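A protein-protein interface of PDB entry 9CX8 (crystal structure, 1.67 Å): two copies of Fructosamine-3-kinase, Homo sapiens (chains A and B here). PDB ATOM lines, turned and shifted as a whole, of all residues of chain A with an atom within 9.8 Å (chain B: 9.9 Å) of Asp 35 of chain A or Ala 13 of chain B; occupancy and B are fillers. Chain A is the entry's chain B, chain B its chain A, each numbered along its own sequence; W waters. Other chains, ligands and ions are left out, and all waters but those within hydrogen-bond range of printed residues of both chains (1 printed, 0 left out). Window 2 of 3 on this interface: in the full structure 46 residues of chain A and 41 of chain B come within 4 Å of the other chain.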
ATOM      1  N   TYR A  32      12.289 -31.172  27.595  1.00  0.00           N
ATOM      2  CA  TYR A  32      11.073 -30.555  28.116  1.00  0.00           C
ATOM      3  C   TYR A  32       9.896 -31.482  27.896  1.00  0.00           C
ATOM      4  O   TYR A  32       9.767 -32.114  26.838  1.00  0.00           O
ATOM      5  CB  TYR A  32      10.752 -29.237  27.419  1.00  0.00           C
ATOM      6  CG  TYR A  32      11.743 -28.140  27.541  1.00  0.00           C
ATOM      7  CD1 TYR A  32      11.665 -27.215  28.579  1.00  0.00           C
ATOM      8  CD2 TYR A  32      12.737 -27.973  26.586  1.00  0.00           C
ATOM      9  CE1 TYR A  32      12.563 -26.165  28.658  1.00  0.00           C
ATOM     10  CE2 TYR A  32      13.623 -26.953  26.651  1.00  0.00           C
ATOM     11  CZ  TYR A  32      13.540 -26.026  27.672  1.00  0.00           C
ATOM     12  OH  TYR A  32      14.443 -24.994  27.746  1.00  0.00           O
ATOM     13  N   ASP A  33       8.978 -31.493  28.861  1.00  0.00           N
ATOM     14  CA  ASP A  33       7.711 -32.133  28.618  1.00  0.00           C
ATOM     15  C   ASP A  33       6.773 -31.078  28.035  1.00  0.00           C
ATOM     16  O   ASP A  33       6.823 -29.913  28.436  1.00  0.00           O
ATOM     17  CB  ASP A  33       7.154 -32.681  29.928  1.00  0.00           C
ATOM     18  CG  ASP A  33       6.276 -33.874  29.711  1.00  0.00           C
ATOM     19  OD1 ASP A  33       5.865 -34.461  30.754  1.00  0.00           O
ATOM     20  OD2 ASP A  33       6.009 -34.226  28.536  1.00  0.00           O
ATOM     21  N   THR A  34       5.947 -31.491  27.096  1.00  0.00           N
ATOM     22  CA  THR A  34       4.998 -30.611  26.430  1.00  0.00           C
ATOM     23  C   THR A  34       3.638 -31.284  26.357  1.00  0.00           C
ATOM     24  O   THR A  34       3.499 -32.484  26.623  1.00  0.00           O
ATOM     25  CB  THR A  34       5.425 -30.258  25.004  1.00  0.00           C
ATOM     26  OG1 THR A  34       5.088 -31.338  24.146  1.00  0.00           O
ATOM     27  CG2 THR A  34       6.946 -29.958  24.898  1.00  0.00           C
ATOM     28  N   ASP A  35       2.640 -30.495  25.929  1.00  0.00           N
ATOM     29  CA  ASP A  35       1.281 -31.022  25.746  1.00  0.00           C
ATOM     30  C   ASP A  35       1.262 -32.310  24.919  1.00  0.00           C
ATOM     31  O   ASP A  35       0.388 -33.156  25.127  1.00  0.00           O
ATOM     32  CB  ASP A  35       0.390 -29.975  25.067  1.00  0.00           C
ATOM     33  CG  ASP A  35       0.119 -28.764  25.939  1.00  0.00           C
ATOM     34  OD1 ASP A  35       0.534 -28.711  27.126  1.00  0.00           O
ATOM     35  OD2 ASP A  35      -0.481 -27.807  25.404  1.00  0.00           O
ATOM     36  N   ALA A  36       2.200 -32.479  23.978  1.00  0.00           N
ATOM     37  CA  ALA A  36       2.242 -33.641  23.089  1.00  0.00           C
ATOM     38  C   ALA A  36       3.349 -34.634  23.438  1.00  0.00           C
ATOM     39  O   ALA A  36       3.716 -35.462  22.592  1.00  0.00           O
ATOM     40  CB  ALA A  36       2.415 -33.216  21.633  1.00  0.00           C
ATOM     41  N   GLY A  37       3.918 -34.556  24.636  1.00  0.00           N
ATOM     42  CA  GLY A  37       5.014 -35.444  24.991  1.00  0.00           C
ATOM     43  C   GLY A  37       6.367 -34.751  25.109  1.00  0.00           C
ATOM     44  O   GLY A  37       6.499 -33.551  24.855  1.00  0.00           O
ATOM     45  N   PRO A  38       7.399 -35.494  25.503  1.00  0.00           N
ATOM     46  CA  PRO A  38       8.717 -34.877  25.700  1.00  0.00           C
ATOM     47  C   PRO A  38       9.445 -34.630  24.396  1.00  0.00           C
ATOM     48  O   PRO A  38       9.274 -35.336  23.401  1.00  0.00           O
ATOM     49  CB  PRO A  38       9.469 -35.910  26.548  1.00  0.00           C
ATOM     50  CG  PRO A  38       8.862 -37.202  26.152  1.00  0.00           C
ATOM     51  CD  PRO A  38       7.385 -36.904  25.934  1.00  0.00           C
ATOM     52  N   VAL A  39      10.315 -33.621  24.435  1.00  0.00           N
ATOM     53  CA  VAL A  39      11.170 -33.268  23.314  1.00  0.00           C
ATOM     54  C   VAL A  39      12.532 -32.934  23.888  1.00  0.00           C
ATOM     55  O   VAL A  39      12.689 -32.724  25.079  1.00  0.00           O
ATOM     56  CB  VAL A  39      10.650 -32.055  22.479  1.00  0.00           C
ATOM     57  CG1 VAL A  39       9.301 -32.376  21.817  1.00  0.00           C
ATOM     58  CG2 VAL A  39      10.580 -30.797  23.337  1.00  0.00           C
ATOM     59  N   GLU B   3      11.727 -19.957  26.160  1.00  0.00           N
ATOM     60  CA  GLU B   3      10.615 -20.865  26.471  1.00  0.00           C
ATOM     61  C   GLU B   3       9.304 -20.429  25.817  1.00  0.00           C
ATOM     62  O   GLU B   3       8.467 -21.268  25.455  1.00  0.00           O
ATOM     63  CB  GLU B   3      10.434 -20.952  27.986  1.00  0.00           C
ATOM     64  CG  GLU B   3      11.651 -21.588  28.709  1.00  0.00           C
ATOM     65  CD  GLU B   3      11.325 -22.037  30.132  1.00  0.00           C
ATOM     66  OE1 GLU B   3      12.066 -21.626  31.047  1.00  0.00           O
ATOM     67  OE2 GLU B   3      10.335 -22.792  30.343  1.00  0.00           O
ATOM     68  N   GLN B   4       9.073 -19.115  25.716  1.00  0.00           N
ATOM     69  CA  GLN B   4       7.895 -18.636  25.004  1.00  0.00           C
ATOM     70  C   GLN B   4       8.001 -18.955  23.512  1.00  0.00           C
ATOM     71  O   GLN B   4       7.015 -19.363  22.885  1.00  0.00           O
ATOM     72  CB  GLN B   4       7.716 -17.125  25.260  1.00  0.00           C
ATOM     73  CG  GLN B   4       7.158 -16.819  26.660  1.00  0.00           C
ATOM     74  CD  GLN B   4       8.249 -16.759  27.746  1.00  0.00           C
ATOM     75  OE1 GLN B   4       9.461 -16.691  27.456  1.00  0.00           O
ATOM     76  NE2 GLN B   4       7.820 -16.845  29.005  1.00  0.00           N
ATOM     77  N   LEU B   6       9.646 -21.500  22.204  1.00  0.00           N
ATOM     78  CA  LEU B   6       9.416 -22.932  22.031  1.00  0.00           C
ATOM     79  C   LEU B   6       7.933 -23.247  22.166  1.00  0.00           C
ATOM     80  O   LEU B   6       7.389 -24.041  21.397  1.00  0.00           O
ATOM     81  CB  LEU B   6      10.197 -23.737  23.080  1.00  0.00           C
ATOM     82  CG  LEU B   6      11.712 -23.784  22.857  1.00  0.00           C
ATOM     83  CD1 LEU B   6      12.429 -24.448  24.052  1.00  0.00           C
ATOM     84  CD2 LEU B   6      12.035 -24.537  21.553  1.00  0.00           C
ATOM     85  N   ARG B   7       7.253 -22.642  23.165  1.00  0.00           N
ATOM     86  CA  ARG B   7       5.813 -22.931  23.300  1.00  0.00           C
ATOM     87  C   ARG B   7       5.051 -22.528  22.039  1.00  0.00           C
ATOM     88  O   ARG B   7       4.176 -23.262  21.563  1.00  0.00           O
ATOM     89  CB  ARG B   7       5.212 -22.219  24.512  1.00  0.00           C
ATOM     90  CG  ARG B   7       5.675 -22.746  25.870  1.00  0.00           C
ATOM     91  CD  ARG B   7       4.912 -22.037  27.032  1.00  0.00           C
ATOM     92  NE  ARG B   7       5.716 -21.970  28.248  1.00  0.00           N
ATOM     93  CZ  ARG B   7       5.484 -22.670  29.352  1.00  0.00           C
ATOM     94  NH1 ARG B   7       6.333 -22.649  30.375  1.00  0.00           N
ATOM     95  NH2 ARG B   7       4.383 -23.417  29.428  1.00  0.00           N
ATOM     96  N   ALA B   8       5.403 -21.380  21.458  1.00  0.00           N
ATOM     97  CA  ALA B   8       4.726 -20.934  20.242  1.00  0.00           C
ATOM     98  C   ALA B   8       5.040 -21.854  19.064  1.00  0.00           C
ATOM     99  O   ALA B   8       4.141 -22.256  18.305  1.00  0.00           O
ATOM    100  CB  ALA B   8       5.163 -19.500  19.925  1.00  0.00           C
ATOM    101  N   GLU B   9       6.331 -22.179  18.874  1.00  0.00           N
ATOM    102  CA  GLU B   9       6.703 -22.965  17.689  1.00  0.00           C
ATOM    103  C   GLU B   9       6.196 -24.400  17.793  1.00  0.00           C
ATOM    104  O   GLU B   9       5.850 -25.012  16.769  1.00  0.00           O
ATOM    105  CB  GLU B   9       8.225 -22.913  17.466  1.00  0.00           C
ATOM    106  CG  GLU B   9       8.757 -21.499  17.232  1.00  0.00           C
ATOM    107  CD  GLU B   9       8.774 -21.099  15.762  1.00  0.00           C
ATOM    108  OE1 GLU B   9       8.502 -21.978  14.904  1.00  0.00           O
ATOM    109  OE2 GLU B   9       9.061 -19.901  15.482  1.00  0.00           O
ATOM    110  N   LEU B  10       6.105 -24.938  19.000  1.00  0.00           N
ATOM    111  CA  LEU B  10       5.622 -26.292  19.190  1.00  0.00           C
ATOM    112  C   LEU B  10       4.139 -26.322  19.490  1.00  0.00           C
ATOM    113  O   LEU B  10       3.585 -27.416  19.679  1.00  0.00           O
ATOM    114  CB  LEU B  10       6.344 -27.002  20.335  1.00  0.00           C
ATOM    115  CG  LEU B  10       7.841 -27.151  20.096  1.00  0.00           C
ATOM    116  CD1 LEU B  10       8.487 -27.654  21.388  1.00  0.00           C
ATOM    117  CD2 LEU B  10       8.141 -28.092  18.943  1.00  0.00           C
ATOM    118  N   ARG B  11       3.507 -25.153  19.583  1.00  0.00           N
ATOM    119  CA  ARG B  11       2.088 -25.037  19.942  1.00  0.00           C
ATOM    120  C   ARG B  11       1.765 -25.864  21.180  1.00  0.00           C
ATOM    121  O   ARG B  11       1.000 -26.828  21.138  1.00  0.00           O
ATOM    122  CB  ARG B  11       1.218 -25.447  18.763  1.00  0.00           C
ATOM    123  CG  ARG B  11       1.398 -24.529  17.563  1.00  0.00           C
ATOM    124  CD  ARG B  11       0.787 -25.102  16.296  1.00  0.00           C
ATOM    125  NE  ARG B  11       1.034 -24.234  15.155  1.00  0.00           N
ATOM    126  CZ  ARG B  11       0.113 -23.500  14.546  1.00  0.00           C
ATOM    127  NH1 ARG B  11      -1.168 -23.574  14.883  1.00  0.00           N
ATOM    128  NH2 ARG B  11       0.485 -22.698  13.552  1.00  0.00           N
ATOM    129  N   THR B  12       2.378 -25.484  22.293  1.00  0.00           N
ATOM    130  CA  THR B  12       2.122 -26.186  23.531  1.00  0.00           C
ATOM    131  C   THR B  12       1.942 -25.209  24.671  1.00  0.00           C
ATOM    132  O   THR B  12       2.615 -24.170  24.744  1.00  0.00           O
ATOM    133  CB  THR B  12       3.248 -27.191  23.862  1.00  0.00           C
ATOM    134  OG1 THR B  12       2.994 -27.769  25.147  1.00  0.00           O
ATOM    135  CG2 THR B  12       4.601 -26.512  23.900  1.00  0.00           C
ATOM    136  N   ALA B  13       1.022 -25.557  25.575  1.00  0.00           N
ATOM    137  CA  ALA B  13       0.816 -24.746  26.765  1.00  0.00           C
ATOM    138  C   ALA B  13       1.869 -25.045  27.827  1.00  0.00           C
ATOM    139  O   ALA B  13       2.407 -24.125  28.453  1.00  0.00           O
ATOM    140  CB  ALA B  13      -0.599 -24.977  27.306  1.00  0.00           C
ATOM    141  N   THR B  14       2.203 -26.315  28.021  1.00  0.00           N
ATOM    142  CA  THR B  14       3.203 -26.725  28.994  1.00  0.00           C
ATOM    143  C   THR B  14       4.571 -26.886  28.328  1.00  0.00           C
ATOM    144  O   THR B  14       4.688 -27.285  27.166  1.00  0.00           O
ATOM    145  CB  THR B  14       2.785 -28.036  29.676  1.00  0.00           C
ATOM    146  OG1 THR B  14       2.704 -29.081  28.692  1.00  0.00           O
ATOM    147  CG2 THR B  14       1.422 -27.872  30.362  1.00  0.00           C
ATOM    148  N   LEU B  15       5.600 -26.550  29.087  1.00  0.00           N
ATOM    149  CA  LEU B  15       6.982 -26.699  28.672  1.00  0.00           C
ATOM    150  C   LEU B  15       7.777 -26.869  29.963  1.00  0.00           C
ATOM    151  O   LEU B  15       8.429 -25.940  30.461  1.00  0.00           O
ATOM    152  CB  LEU B  15       7.494 -25.508  27.878  1.00  0.00           C
ATOM    153  CG  LEU B  15       8.786 -25.763  27.113  1.00  0.00           C
ATOM    154  CD1 LEU B  15       8.474 -26.500  25.813  1.00  0.00           C
ATOM    155  CD2 LEU B  15       9.495 -24.416  26.912  1.00  0.00           C
ATOM    156  N   ARG B  16       7.720 -28.081  30.498  1.00  0.00           N
ATOM    157  CA  ARG B  16       8.285 -28.385  31.802  1.00  0.00           C
ATOM    158  C   ARG B  16       9.628 -29.053  31.590  1.00  0.00           C
ATOM    159  O   ARG B  16       9.677 -30.216  31.170  1.00  0.00           O
ATOM    160  CB  ARG B  16       7.351 -29.301  32.593  1.00  0.00           C
ATOM    161  CG  ARG B  16       7.904 -29.672  33.957  1.00  0.00           C
ATOM    162  CD  ARG B  16       6.916 -30.525  34.733  1.00  0.00           C
ATOM    163  NE  ARG B  16       7.005 -31.927  34.340  1.00  0.00           N
ATOM    164  CZ  ARG B  16       8.021 -32.737  34.625  1.00  0.00           C
ATOM    165  NH1 ARG B  16       9.074 -32.321  35.322  1.00  0.00           N
ATOM    166  NH2 ARG B  16       7.980 -33.998  34.199  1.00  0.00           N
HETATM  167  O   HOH W   1      14.199 -23.290  29.515  1.00  0.00           O
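Water W1 bridges the side-chain hydroxyl of Tyr 32 of chain A (2.5 Å) and the side-chain carboxylate of Glu 3 of chain B (3.1 Å).
Of the 8 printed residues of chain A, 4 touch a printed residue of chain B.
Hydrophobic or aromatic side chains of chain A within 4 Å of the printed part of chain B: Tyr 32.
Hydrophobic or aromatic side chains of chain B within 4 Å of the printed part of chain A: Leu 6, Ala 13 and Leu 15.
Among the printed residues, no Asp or Glu carboxylate lies within 4 Å of a Lys or Arg side-chain nitrogen of the other chain.
Printed residues of chain B within 4 Å of Tyr 32 of chain A: Leu 6 (3.8 Å), Leu 15 (3.5 Å) and Arg 16 (3.4 Å).
Of the printed residues of chain B, Asp 33 of chain A touches Thr 14, Leu 15 and Arg 16.
Thr 34 of chain A touches three residues of chain B.
Asp 35 of chain A touches just these residues of chain B: Thr 12 (2.9 Å), Ala 13 (2.7 Å) and Thr 14 (2.7 Å).
No residue of chain B comes within 4 Å of Ala 36 of chain A.
No residue of chain B comes within 4 Å of Gly 37 of chain A.
Gln 4 of chain B touches none of the printed residues of chain A.
Of the printed residues of chain A, Leu 6 of chain B touches Tyr 32 (3.8 Å).
Arg 7 of chain B touches none of the printed residues of chain A.
Ala 13 of chain B touches just one residue of chain A: Asp 35.
Printed residues of chain A within 4 Å of Leu 15 of chain B: Tyr 32, Asp 33 and Thr 34.
Printed residues of chain A within 4 Å of Arg 16 of chain B: Tyr 32 (3.4 Å) and Asp 33 (2.7 Å).
The nearest residue of chain A that does not touch Ala 13 of chain B is Thr 34 of chain A (6.3 Å).
The nearest printed residue of chain B that does not touch Tyr 32 of chain A is Glu 3 of chain B (4.4 Å).
No position is printed for both chains.
Of the 12 pairs that touch across the chains among the printed residues, none has its exchanged pair printed and touching as well.
The backbone carbonyl oxygen of Gly 37 of chain A is in hydrogen-bond range of the side-chain hydroxyl of Thr 34 of chain A (2.7 Å).
The backbone NH of Thr 12 of chain B lies within hydrogen-bond range of the backbone carbonyl oxygen of Arg 7 of chain B (3.0 Å).
N of Val 39 of chain A is in hydrogen-bond range of O of Tyr 32 of chain A (2.9 Å).
The backbone carbonyl oxygen (O) of Thr 14 of chain B is in hydrogen-bond range of the side-chain hydroxyl (OG1) of Thr 12 of chain B (2.7 Å).
The side-chain hydroxyl (OG1) of Thr 34 of chain A sits close to the backbone NH (N) of Ala 36 of chain A, 3.1 Å away.
Among the printed residues, pairs that only touch across the chains: Asp 33 of chain A with Leu 15 of chain B (3.2 Å), Thr 34 of chain A with Thr 14 of chain B (3.3 Å), Tyr 32 of chain A with Arg 16 of chain B (3.4 Å), Thr 34 of chain A with Thr 12 of chain B (3.5 Å), Tyr 32 of chain A with Leu 15 of chain B (3.5 Å), Asp 33 of chain A with Thr 14 of chain B (3.6 Å), Tyr 32 of chain A with Leu 6 of chain B (3.8 Å) and Thr 34 of chain A with Leu 15 of chain B (3.9 Å).
The side-chain hydroxyl (OG1) of Thr 14 of chain B is in hydrogen-bond range of the side-chain carboxylate (OD1) of Asp 35 of chain A, at 2.7 Å.
The side-chain hydroxyl of Thr 12 of chain B sits at hydrogen-bond distance from the backbone NH of Asp 35 of chain A (2.9 Å).
The backbone NH of Ala 13 of chain B lies within hydrogen-bond range of the side-chain carboxylate of Asp 35 of chain A.
The backbone carbonyl oxygen of Arg 16 of chain B lies within hydrogen-bond range of the backbone NH of Asp 33 of chain A, at 2.7 Å.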
